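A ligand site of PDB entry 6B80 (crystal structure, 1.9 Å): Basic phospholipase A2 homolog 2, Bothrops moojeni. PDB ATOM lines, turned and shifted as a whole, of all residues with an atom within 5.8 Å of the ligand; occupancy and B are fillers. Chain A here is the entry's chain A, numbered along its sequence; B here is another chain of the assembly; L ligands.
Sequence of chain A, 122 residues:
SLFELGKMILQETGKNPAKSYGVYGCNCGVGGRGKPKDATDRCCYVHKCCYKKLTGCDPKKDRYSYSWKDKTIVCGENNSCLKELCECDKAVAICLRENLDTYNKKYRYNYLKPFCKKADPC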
ATOM      1  N   LEU A   2      25.764  -0.238 -25.310  1.00  0.00           N
ATOM      2  CA  LEU A   2      24.756   0.836 -25.296  1.00  0.00           C
ATOM      3  C   LEU A   2      24.584   1.449 -23.905  1.00  0.00           C
ATOM      4  O   LEU A   2      24.294   2.642 -23.783  1.00  0.00           O
ATOM      5  CB  LEU A   2      23.405   0.300 -25.760  1.00  0.00           C
ATOM      6  CG  LEU A   2      23.267  -0.066 -27.225  1.00  0.00           C
ATOM      7  CD1 LEU A   2      21.782  -0.350 -27.496  1.00  0.00           C
ATOM      8  CD2 LEU A   2      23.780   1.025 -28.132  1.00  0.00           C
ATOM      9  N   PHE A   3      24.728   0.630 -22.869  1.00  0.00           N
ATOM     10  CA  PHE A   3      24.648   1.175 -21.530  1.00  0.00           C
ATOM     11  C   PHE A   3      25.692   2.287 -21.282  1.00  0.00           C
ATOM     12  O   PHE A   3      25.343   3.445 -20.930  1.00  0.00           O
ATOM     13  CB  PHE A   3      24.767   0.061 -20.515  1.00  0.00           C
ATOM     14  CG  PHE A   3      24.804   0.536 -19.107  1.00  0.00           C
ATOM     15  CD1 PHE A   3      23.629   0.928 -18.472  1.00  0.00           C
ATOM     16  CD2 PHE A   3      26.011   0.623 -18.420  1.00  0.00           C
ATOM     17  CE1 PHE A   3      23.648   1.393 -17.168  1.00  0.00           C
ATOM     18  CE2 PHE A   3      26.041   1.083 -17.112  1.00  0.00           C
ATOM     19  CZ  PHE A   3      24.851   1.470 -16.482  1.00  0.00           C
ATOM     20  N   LEU A   5      27.397   3.881 -23.453  1.00  0.00           N
ATOM     21  CA  LEU A   5      27.239   4.962 -24.435  1.00  0.00           C
ATOM     22  C   LEU A   5      26.136   5.931 -24.013  1.00  0.00           C
ATOM     23  O   LEU A   5      26.330   7.149 -24.018  1.00  0.00           O
ATOM     24  CB  LEU A   5      26.985   4.376 -25.824  1.00  0.00           C
ATOM     25  CG  LEU A   5      26.554   5.288 -26.963  1.00  0.00           C
ATOM     26  CD1 LEU A   5      27.668   6.309 -27.225  1.00  0.00           C
ATOM     27  CD2 LEU A   5      26.278   4.450 -28.201  1.00  0.00           C
ATOM     28  N   GLY A   6      24.969   5.401 -23.626  1.00  0.00           N
ATOM     29  CA  GLY A   6      23.866   6.265 -23.212  1.00  0.00           C
ATOM     30  C   GLY A   6      24.217   7.058 -21.959  1.00  0.00           C
ATOM     31  O   GLY A   6      23.835   8.227 -21.823  1.00  0.00           O
ATOM     32  N   ILE A   9      26.545   9.960 -22.901  1.00  0.00           N
ATOM     33  CA  ILE A   9      25.777  11.005 -23.559  1.00  0.00           C
ATOM     34  C   ILE A   9      24.999  11.853 -22.537  1.00  0.00           C
ATOM     35  O   ILE A   9      25.021  13.085 -22.598  1.00  0.00           O
ATOM     36  CB  ILE A   9      24.871  10.427 -24.665  1.00  0.00           C
ATOM     37  CG1 ILE A   9      25.764   9.883 -25.792  1.00  0.00           C
ATOM     38  CG2 ILE A   9      23.904  11.494 -25.201  1.00  0.00           C
ATOM     39  CD1 ILE A   9      25.032   9.083 -26.881  1.00  0.00           C
ATOM     40  N   PRO A  17      19.457  10.374 -23.380  1.00  0.00           N
ATOM     41  CA  PRO A  17      20.140  10.060 -24.651  1.00  0.00           C
ATOM     42  C   PRO A  17      19.237   9.394 -25.696  1.00  0.00           C
ATOM     43  O   PRO A  17      19.286   9.793 -26.871  1.00  0.00           O
ATOM     44  CB  PRO A  17      21.262   9.095 -24.208  1.00  0.00           C
ATOM     45  CG  PRO A  17      20.799   8.522 -22.864  1.00  0.00           C
ATOM     46  CD  PRO A  17      20.029   9.649 -22.225  1.00  0.00           C
ATOM     47  N   ALA A  18      18.449   8.392 -25.317  1.00  0.00           N
ATOM     48  CA  ALA A  18      17.565   7.749 -26.290  1.00  0.00           C
ATOM     49  C   ALA A  18      16.548   8.746 -26.772  1.00  0.00           C
ATOM     50  O   ALA A  18      16.145   8.760 -27.943  1.00  0.00           O
ATOM     51  CB  ALA A  18      16.861   6.541 -25.664  1.00  0.00           C
ATOM     52  N   TYR A  21      18.565  11.412 -29.069  1.00  0.00           N
ATOM     53  CA  TYR A  21      19.440  10.923 -30.123  1.00  0.00           C
ATOM     54  C   TYR A  21      19.101   9.535 -30.650  1.00  0.00           C
ATOM     55  O   TYR A  21      19.779   9.056 -31.550  1.00  0.00           O
ATOM     56  CB  TYR A  21      20.889  10.956 -29.639  1.00  0.00           C
ATOM     57  CG  TYR A  21      21.312  12.341 -29.150  1.00  0.00           C
ATOM     58  CD1 TYR A  21      21.498  12.594 -27.803  1.00  0.00           C
ATOM     59  CD2 TYR A  21      21.523  13.379 -30.057  1.00  0.00           C
ATOM     60  CE1 TYR A  21      21.854  13.845 -27.353  1.00  0.00           C
ATOM     61  CE2 TYR A  21      21.903  14.634 -29.628  1.00  0.00           C
ATOM     62  CZ  TYR A  21      22.067  14.862 -28.265  1.00  0.00           C
ATOM     63  OH  TYR A  21      22.441  16.097 -27.814  1.00  0.00           O
ATOM     64  N   GLY A  22      18.081   8.889 -30.105  1.00  0.00           N
ATOM     65  CA  GLY A  22      17.766   7.530 -30.527  1.00  0.00           C
ATOM     66  C   GLY A  22      17.308   7.418 -31.973  1.00  0.00           C
ATOM     67  O   GLY A  22      17.456   6.356 -32.607  1.00  0.00           O
ATOM     68  N   ASN A  27      21.866   9.881 -38.966  1.00  0.00           N
ATOM     69  CA  ASN A  27      23.000   9.148 -38.397  1.00  0.00           C
ATOM     70  C   ASN A  27      22.916   8.735 -36.934  1.00  0.00           C
ATOM     71  O   ASN A  27      23.636   7.832 -36.505  1.00  0.00           O
ATOM     72  CB  ASN A  27      24.283   9.947 -38.608  1.00  0.00           C
ATOM     73  CG  ASN A  27      24.645  10.076 -40.067  1.00  0.00           C
ATOM     74  OD1 ASN A  27      25.285   9.173 -40.631  1.00  0.00           O
ATOM     75  ND2 ASN A  27      24.184  11.149 -40.699  1.00  0.00           N
ATOM     76  N   CYS A  28      22.090   9.421 -36.152  1.00  0.00           N
ATOM     77  CA  CYS A  28      22.041   9.166 -34.708  1.00  0.00           C
ATOM     78  C   CYS A  28      21.092   8.037 -34.349  1.00  0.00           C
ATOM     79  O   CYS A  28      19.945   8.025 -34.816  1.00  0.00           O
ATOM     80  CB  CYS A  28      21.629  10.418 -33.948  1.00  0.00           C
ATOM     81  SG  CYS A  28      22.818  11.747 -34.120  1.00  0.00           S
ATOM     82  N   GLY A  29      21.572   7.104 -33.523  1.00  0.00           N
ATOM     83  CA  GLY A  29      20.724   6.099 -32.909  1.00  0.00           C
ATOM     84  C   GLY A  29      20.484   4.908 -33.818  1.00  0.00           C
ATOM     85  O   GLY A  29      21.429   4.408 -34.440  1.00  0.00           O
ATOM     86  N   VAL A  30      19.219   4.474 -33.902  1.00  0.00           N
ATOM     87  CA  VAL A  30      18.852   3.306 -34.686  1.00  0.00           C
ATOM     88  C   VAL A  30      19.278   3.446 -36.137  1.00  0.00           C
ATOM     89  O   VAL A  30      19.416   4.560 -36.646  1.00  0.00           O
ATOM     90  CB  VAL A  30      17.303   3.039 -34.672  1.00  0.00           C
ATOM     91  CG1 VAL A  30      16.782   2.951 -33.258  1.00  0.00           C
ATOM     92  CG2 VAL A  30      16.549   4.136 -35.427  1.00  0.00           C
ATOM     93  N   CYS A  44      27.253  11.752 -34.934  1.00  0.00           N
ATOM     94  CA  CYS A  44      26.840  10.359 -34.900  1.00  0.00           C
ATOM     95  C   CYS A  44      27.397   9.598 -36.097  1.00  0.00           C
ATOM     96  O   CYS A  44      27.738   8.409 -35.999  1.00  0.00           O
ATOM     97  CB  CYS A  44      25.318  10.271 -34.865  1.00  0.00           C
ATOM     98  SG  CYS A  44      24.568  10.993 -33.380  1.00  0.00           S
ATOM     99  N   HIS A  47      30.790   8.707 -35.177  1.00  0.00           N
ATOM    100  CA  HIS A  47      30.706   7.646 -34.185  1.00  0.00           C
ATOM    101  C   HIS A  47      30.451   6.291 -34.842  1.00  0.00           C
ATOM    102  O   HIS A  47      31.081   5.273 -34.483  1.00  0.00           O
ATOM    103  CB  HIS A  47      29.605   7.977 -33.173  1.00  0.00           C
ATOM    104  CG  HIS A  47      29.508   6.977 -32.054  1.00  0.00           C
ATOM    105  ND1 HIS A  47      28.397   6.188 -31.850  1.00  0.00           N
ATOM    106  CD2 HIS A  47      30.386   6.648 -31.069  1.00  0.00           C
ATOM    107  CE1 HIS A  47      28.588   5.417 -30.792  1.00  0.00           C
ATOM    108  NE2 HIS A  47      29.791   5.672 -30.305  1.00  0.00           N
ATOM    109  N   LYS A  48      29.524   6.267 -35.793  1.00  0.00           N
ATOM    110  CA  LYS A  48      29.214   5.035 -36.492  1.00  0.00           C
ATOM    111  C   LYS A  48      30.425   4.546 -37.304  1.00  0.00           C
ATOM    112  O   LYS A  48      30.662   3.347 -37.416  1.00  0.00           O
ATOM    113  CB  LYS A  48      27.942   5.187 -37.360  1.00  0.00           C
ATOM    114  CG  LYS A  48      26.634   4.934 -36.597  1.00  0.00           C
ATOM    115  CD  LYS A  48      25.408   5.126 -37.512  1.00  0.00           C
ATOM    116  CE  LYS A  48      24.105   4.717 -36.813  1.00  0.00           C
ATOM    117  NZ  LYS A  48      23.811   5.567 -35.646  1.00  0.00           N
ATOM    118  N   TYR A  51      32.822   3.019 -34.897  1.00  0.00           N
ATOM    119  CA  TYR A  51      32.375   1.644 -34.613  1.00  0.00           C
ATOM    120  C   TYR A  51      32.790   0.691 -35.707  1.00  0.00           C
ATOM    121  O   TYR A  51      33.154  -0.451 -35.421  1.00  0.00           O
ATOM    122  CB  TYR A  51      30.840   1.585 -34.456  1.00  0.00           C
ATOM    123  CG  TYR A  51      30.342   1.858 -33.064  1.00  0.00           C
ATOM    124  CD1 TYR A  51      31.169   2.468 -32.117  1.00  0.00           C
ATOM    125  CD2 TYR A  51      29.054   1.513 -32.679  1.00  0.00           C
ATOM    126  CE1 TYR A  51      30.710   2.735 -30.853  1.00  0.00           C
ATOM    127  CE2 TYR A  51      28.590   1.750 -31.408  1.00  0.00           C
ATOM    128  CZ  TYR A  51      29.433   2.346 -30.493  1.00  0.00           C
ATOM    129  OH  TYR A  51      28.991   2.607 -29.215  1.00  0.00           O
ATOM    130  N   VAL A  92      31.834  10.736 -29.126  1.00  0.00           N
ATOM    131  CA  VAL A  92      30.510  11.155 -29.570  1.00  0.00           C
ATOM    132  C   VAL A  92      29.746  11.902 -28.484  1.00  0.00           C
ATOM    133  O   VAL A  92      29.075  12.918 -28.759  1.00  0.00           O
ATOM    134  CB  VAL A  92      29.671  10.007 -30.157  1.00  0.00           C
ATOM    135  CG1 VAL A  92      29.056   9.136 -29.044  1.00  0.00           C
ATOM    136  CG2 VAL A  92      28.577  10.617 -31.019  1.00  0.00           C
ATOM    137  N   LEU A  96      28.389  15.545 -29.109  1.00  0.00           N
ATOM    138  CA  LEU A  96      26.973  15.882 -29.009  1.00  0.00           C
ATOM    139  C   LEU A  96      26.750  17.089 -28.095  1.00  0.00           C
ATOM    140  O   LEU A  96      25.946  17.979 -28.380  1.00  0.00           O
ATOM    141  CB  LEU A  96      26.180  14.677 -28.521  1.00  0.00           C
ATOM    142  CG  LEU A  96      26.085  13.508 -29.500  1.00  0.00           C
ATOM    143  CD1 LEU A  96      25.416  12.348 -28.782  1.00  0.00           C
ATOM    144  CD2 LEU A  96      25.289  13.898 -30.731  1.00  0.00           C
ATOM    145  N   VAL B  23      13.133   1.997 -25.157  1.00  0.00           N
ATOM    146  CA  VAL B  23      13.911   1.543 -23.997  1.00  0.00           C
ATOM    147  C   VAL B  23      12.994   1.119 -22.848  1.00  0.00           C
ATOM    148  O   VAL B  23      13.338   1.248 -21.670  1.00  0.00           O
ATOM    149  CB  VAL B  23      14.908   2.628 -23.545  1.00  0.00           C
ATOM    150  CG1 VAL B  23      16.003   2.026 -22.637  1.00  0.00           C
ATOM    151  CG2 VAL B  23      15.547   3.298 -24.771  1.00  0.00           C
ATOM    152  N   VAL B  30      15.825  -1.688 -27.338  1.00  0.00           N
ATOM    153  CA  VAL B  30      17.207  -2.111 -27.384  1.00  0.00           C
ATOM    154  C   VAL B  30      17.470  -3.266 -26.427  1.00  0.00           C
ATOM    155  O   VAL B  30      16.712  -3.479 -25.453  1.00  0.00           O
ATOM    156  CB  VAL B  30      18.134  -0.927 -27.017  1.00  0.00           C
ATOM    157  CG1 VAL B  30      17.928   0.211 -27.990  1.00  0.00           C
ATOM    158  CG2 VAL B  30      17.846  -0.459 -25.591  1.00  0.00           C
ATOM    159  N   ASN B 110      14.268   2.728 -19.482  1.00  0.00           N
ATOM    160  CA  ASN B 110      14.966   1.860 -18.551  1.00  0.00           C
ATOM    161  C   ASN B 110      16.429   1.699 -18.893  1.00  0.00           C
ATOM    162  O   ASN B 110      16.841   0.702 -19.519  1.00  0.00           O
ATOM    163  CB  ASN B 110      14.305   0.480 -18.516  1.00  0.00           C
ATOM    164  CG  ASN B 110      14.894  -0.394 -17.428  1.00  0.00           C
ATOM    165  OD1 ASN B 110      15.583   0.113 -16.518  1.00  0.00           O
ATOM    166  ND2 ASN B 110      14.642  -1.716 -17.506  1.00  0.00           N
ATOM    167  N   TYR B 111      17.239   2.632 -18.454  1.00  0.00           N
ATOM    168  CA  TYR B 111      18.649   2.548 -18.738  1.00  0.00           C
ATOM    169  C   TYR B 111      19.324   1.490 -17.864  1.00  0.00           C
ATOM    170  O   TYR B 111      20.531   1.250 -17.977  1.00  0.00           O
ATOM    171  CB  TYR B 111      19.290   3.924 -18.576  1.00  0.00           C
ATOM    172  CG  TYR B 111      18.830   4.833 -19.680  1.00  0.00           C
ATOM    173  CD1 TYR B 111      19.011   4.466 -21.008  1.00  0.00           C
ATOM    174  CD2 TYR B 111      18.208   6.058 -19.408  1.00  0.00           C
ATOM    175  CE1 TYR B 111      18.582   5.288 -22.042  1.00  0.00           C
ATOM    176  CE2 TYR B 111      17.778   6.879 -20.420  1.00  0.00           C
ATOM    177  CZ  TYR B 111      17.967   6.478 -21.735  1.00  0.00           C
ATOM    178  OH  TYR B 111      17.547   7.266 -22.779  1.00  0.00           O
ATOM    179  N   LEU B 112      18.520   0.847 -17.015  1.00  0.00           N
ATOM    180  CA  LEU B 112      19.010  -0.216 -16.139  1.00  0.00           C
ATOM    181  C   LEU B 112      18.722  -1.596 -16.731  1.00  0.00           C
ATOM    182  O   LEU B 112      18.844  -2.610 -16.052  1.00  0.00           O
ATOM    183  CB  LEU B 112      18.353  -0.083 -14.759  1.00  0.00           C
ATOM    184  CG  LEU B 112      19.097   0.639 -13.645  1.00  0.00           C
ATOM    185  CD1 LEU B 112      20.163   1.584 -14.177  1.00  0.00           C
ATOM    186  CD2 LEU B 112      18.115   1.389 -12.751  1.00  0.00           C
ATOM    187  N   LYS B 113      18.343  -1.636 -18.010  1.00  0.00           N
ATOM    188  CA  LYS B 113      18.174  -2.899 -18.754  1.00  0.00           C
ATOM    189  C   LYS B 113      19.228  -3.999 -18.516  1.00  0.00           C
ATOM    190  O   LYS B 113      18.850  -5.178 -18.391  1.00  0.00           O
ATOM    191  CB  LYS B 113      18.073  -2.636 -20.253  1.00  0.00           C
ATOM    192  CG  LYS B 113      16.664  -2.252 -20.733  1.00  0.00           C
ATOM    193  CD  LYS B 113      16.612  -2.119 -22.244  1.00  0.00           C
ATOM    194  CE  LYS B 113      15.280  -1.580 -22.751  1.00  0.00           C
ATOM    195  NZ  LYS B 113      14.156  -2.577 -22.712  1.00  0.00           N
ATOM    196  N   PRO B 114      20.540  -3.649 -18.523  1.00  0.00           N
ATOM    197  CA  PRO B 114      21.545  -4.711 -18.335  1.00  0.00           C
ATOM    198  C   PRO B 114      21.398  -5.413 -16.996  1.00  0.00           C
ATOM    199  O   PRO B 114      21.965  -6.475 -16.839  1.00  0.00           O
ATOM    200  CB  PRO B 114      22.877  -3.929 -18.293  1.00  0.00           C
ATOM    201  CG  PRO B 114      22.592  -2.662 -19.054  1.00  0.00           C
ATOM    202  CD  PRO B 114      21.157  -2.346 -18.839  1.00  0.00           C
HETATM  203  C1  LIG L   1      25.360   7.036 -32.623  1.00  0.00           C
HETATM  204  O1  LIG L   1      26.323   6.353 -33.077  1.00  0.00           O
HETATM  205  O2  LIG L   1      24.198   7.000 -33.132  1.00  0.00           O
HETATM  206  C2  LIG L   1      25.588   7.911 -31.413  1.00  0.00           C
HETATM  207  C3  LIG L   1      24.333   8.313 -30.664  1.00  0.00           C
HETATM  208  C4  LIG L   1      23.646   7.169 -29.945  1.00  0.00           C
HETATM  209  C5  LIG L   1      22.326   7.607 -29.327  1.00  0.00           C
HETATM  210  C6  LIG L   1      21.692   6.594 -28.409  1.00  0.00           C
HETATM  211  C7  LIG L   1      22.617   6.221 -27.253  1.00  0.00           C
HETATM  212  C8  LIG L   1      22.173   5.008 -26.443  1.00  0.00           C
HETATM  213  C9  LIG L   1      20.709   5.063 -26.064  1.00  0.00           C
HETATM  214  C10 LIG L   1      20.221   3.738 -25.466  1.00  0.00           C
HETATM  215  C11 LIG L   1      20.867   3.400 -24.149  1.00  0.00           C
HETATM  216  C12 LIG L   1      20.228   2.162 -23.513  1.00  0.00           C
HETATM  217  C13 LIG L   1      21.113   1.483 -22.496  1.00  0.00           C
HETATM  218  C14 LIG L   1      20.439   0.267 -21.874  1.00  0.00           C
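Residues that only touch the ligand: Cys 28, Asn 27, Leu 2, Tyr 111 of chain B, Tyr 21, Phe 3, Ile 9, Cys 44 and Gly 6. Hydrophobic or aromatic side chains that line the ligand: Ile 9, Tyr 21, His 47 and Tyr 111 of chain B. Of the 26 residues printed, 12 come within 4 Å of the ligand.
OH of Tyr 51 sits close to NE2 of His 47, 3.3 Å away. The side-chain amino group (NZ) of Lys 48 sits at hydrogen-bond distance from the backbone carbonyl oxygen (O) of Gly 29. N of Gly 29 lies within hydrogen-bond range of O of Tyr 21 (3.3 Å). The side-chain amino group (NZ) of Lys 48 lies within hydrogen-bond range of the backbone carbonyl oxygen (O) of Asn 27 (2.4 Å). SG of Cys 44 is disulfide-bonded to SG of Cys 28 (2.0 Å). The backbone NH (N) of Ala 18 sits at hydrogen-bond distance from the side-chain hydroxyl (OH) of Tyr 111 of chain B, at 2.9 Å.
A ring nitrogen (ND1) of His 47 sits at hydrogen-bond distance from an oxygen (O1) of the ligand, at 2.4 Å. An oxygen (O2) of the ligand sits at hydrogen-bond distance from the backbone NH of Gly 29, at 2.7 Å. The side-chain amino group of Lys 48 lies within salt-bridge range of an oxygen (O2) of the ligand (2.9 Å).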
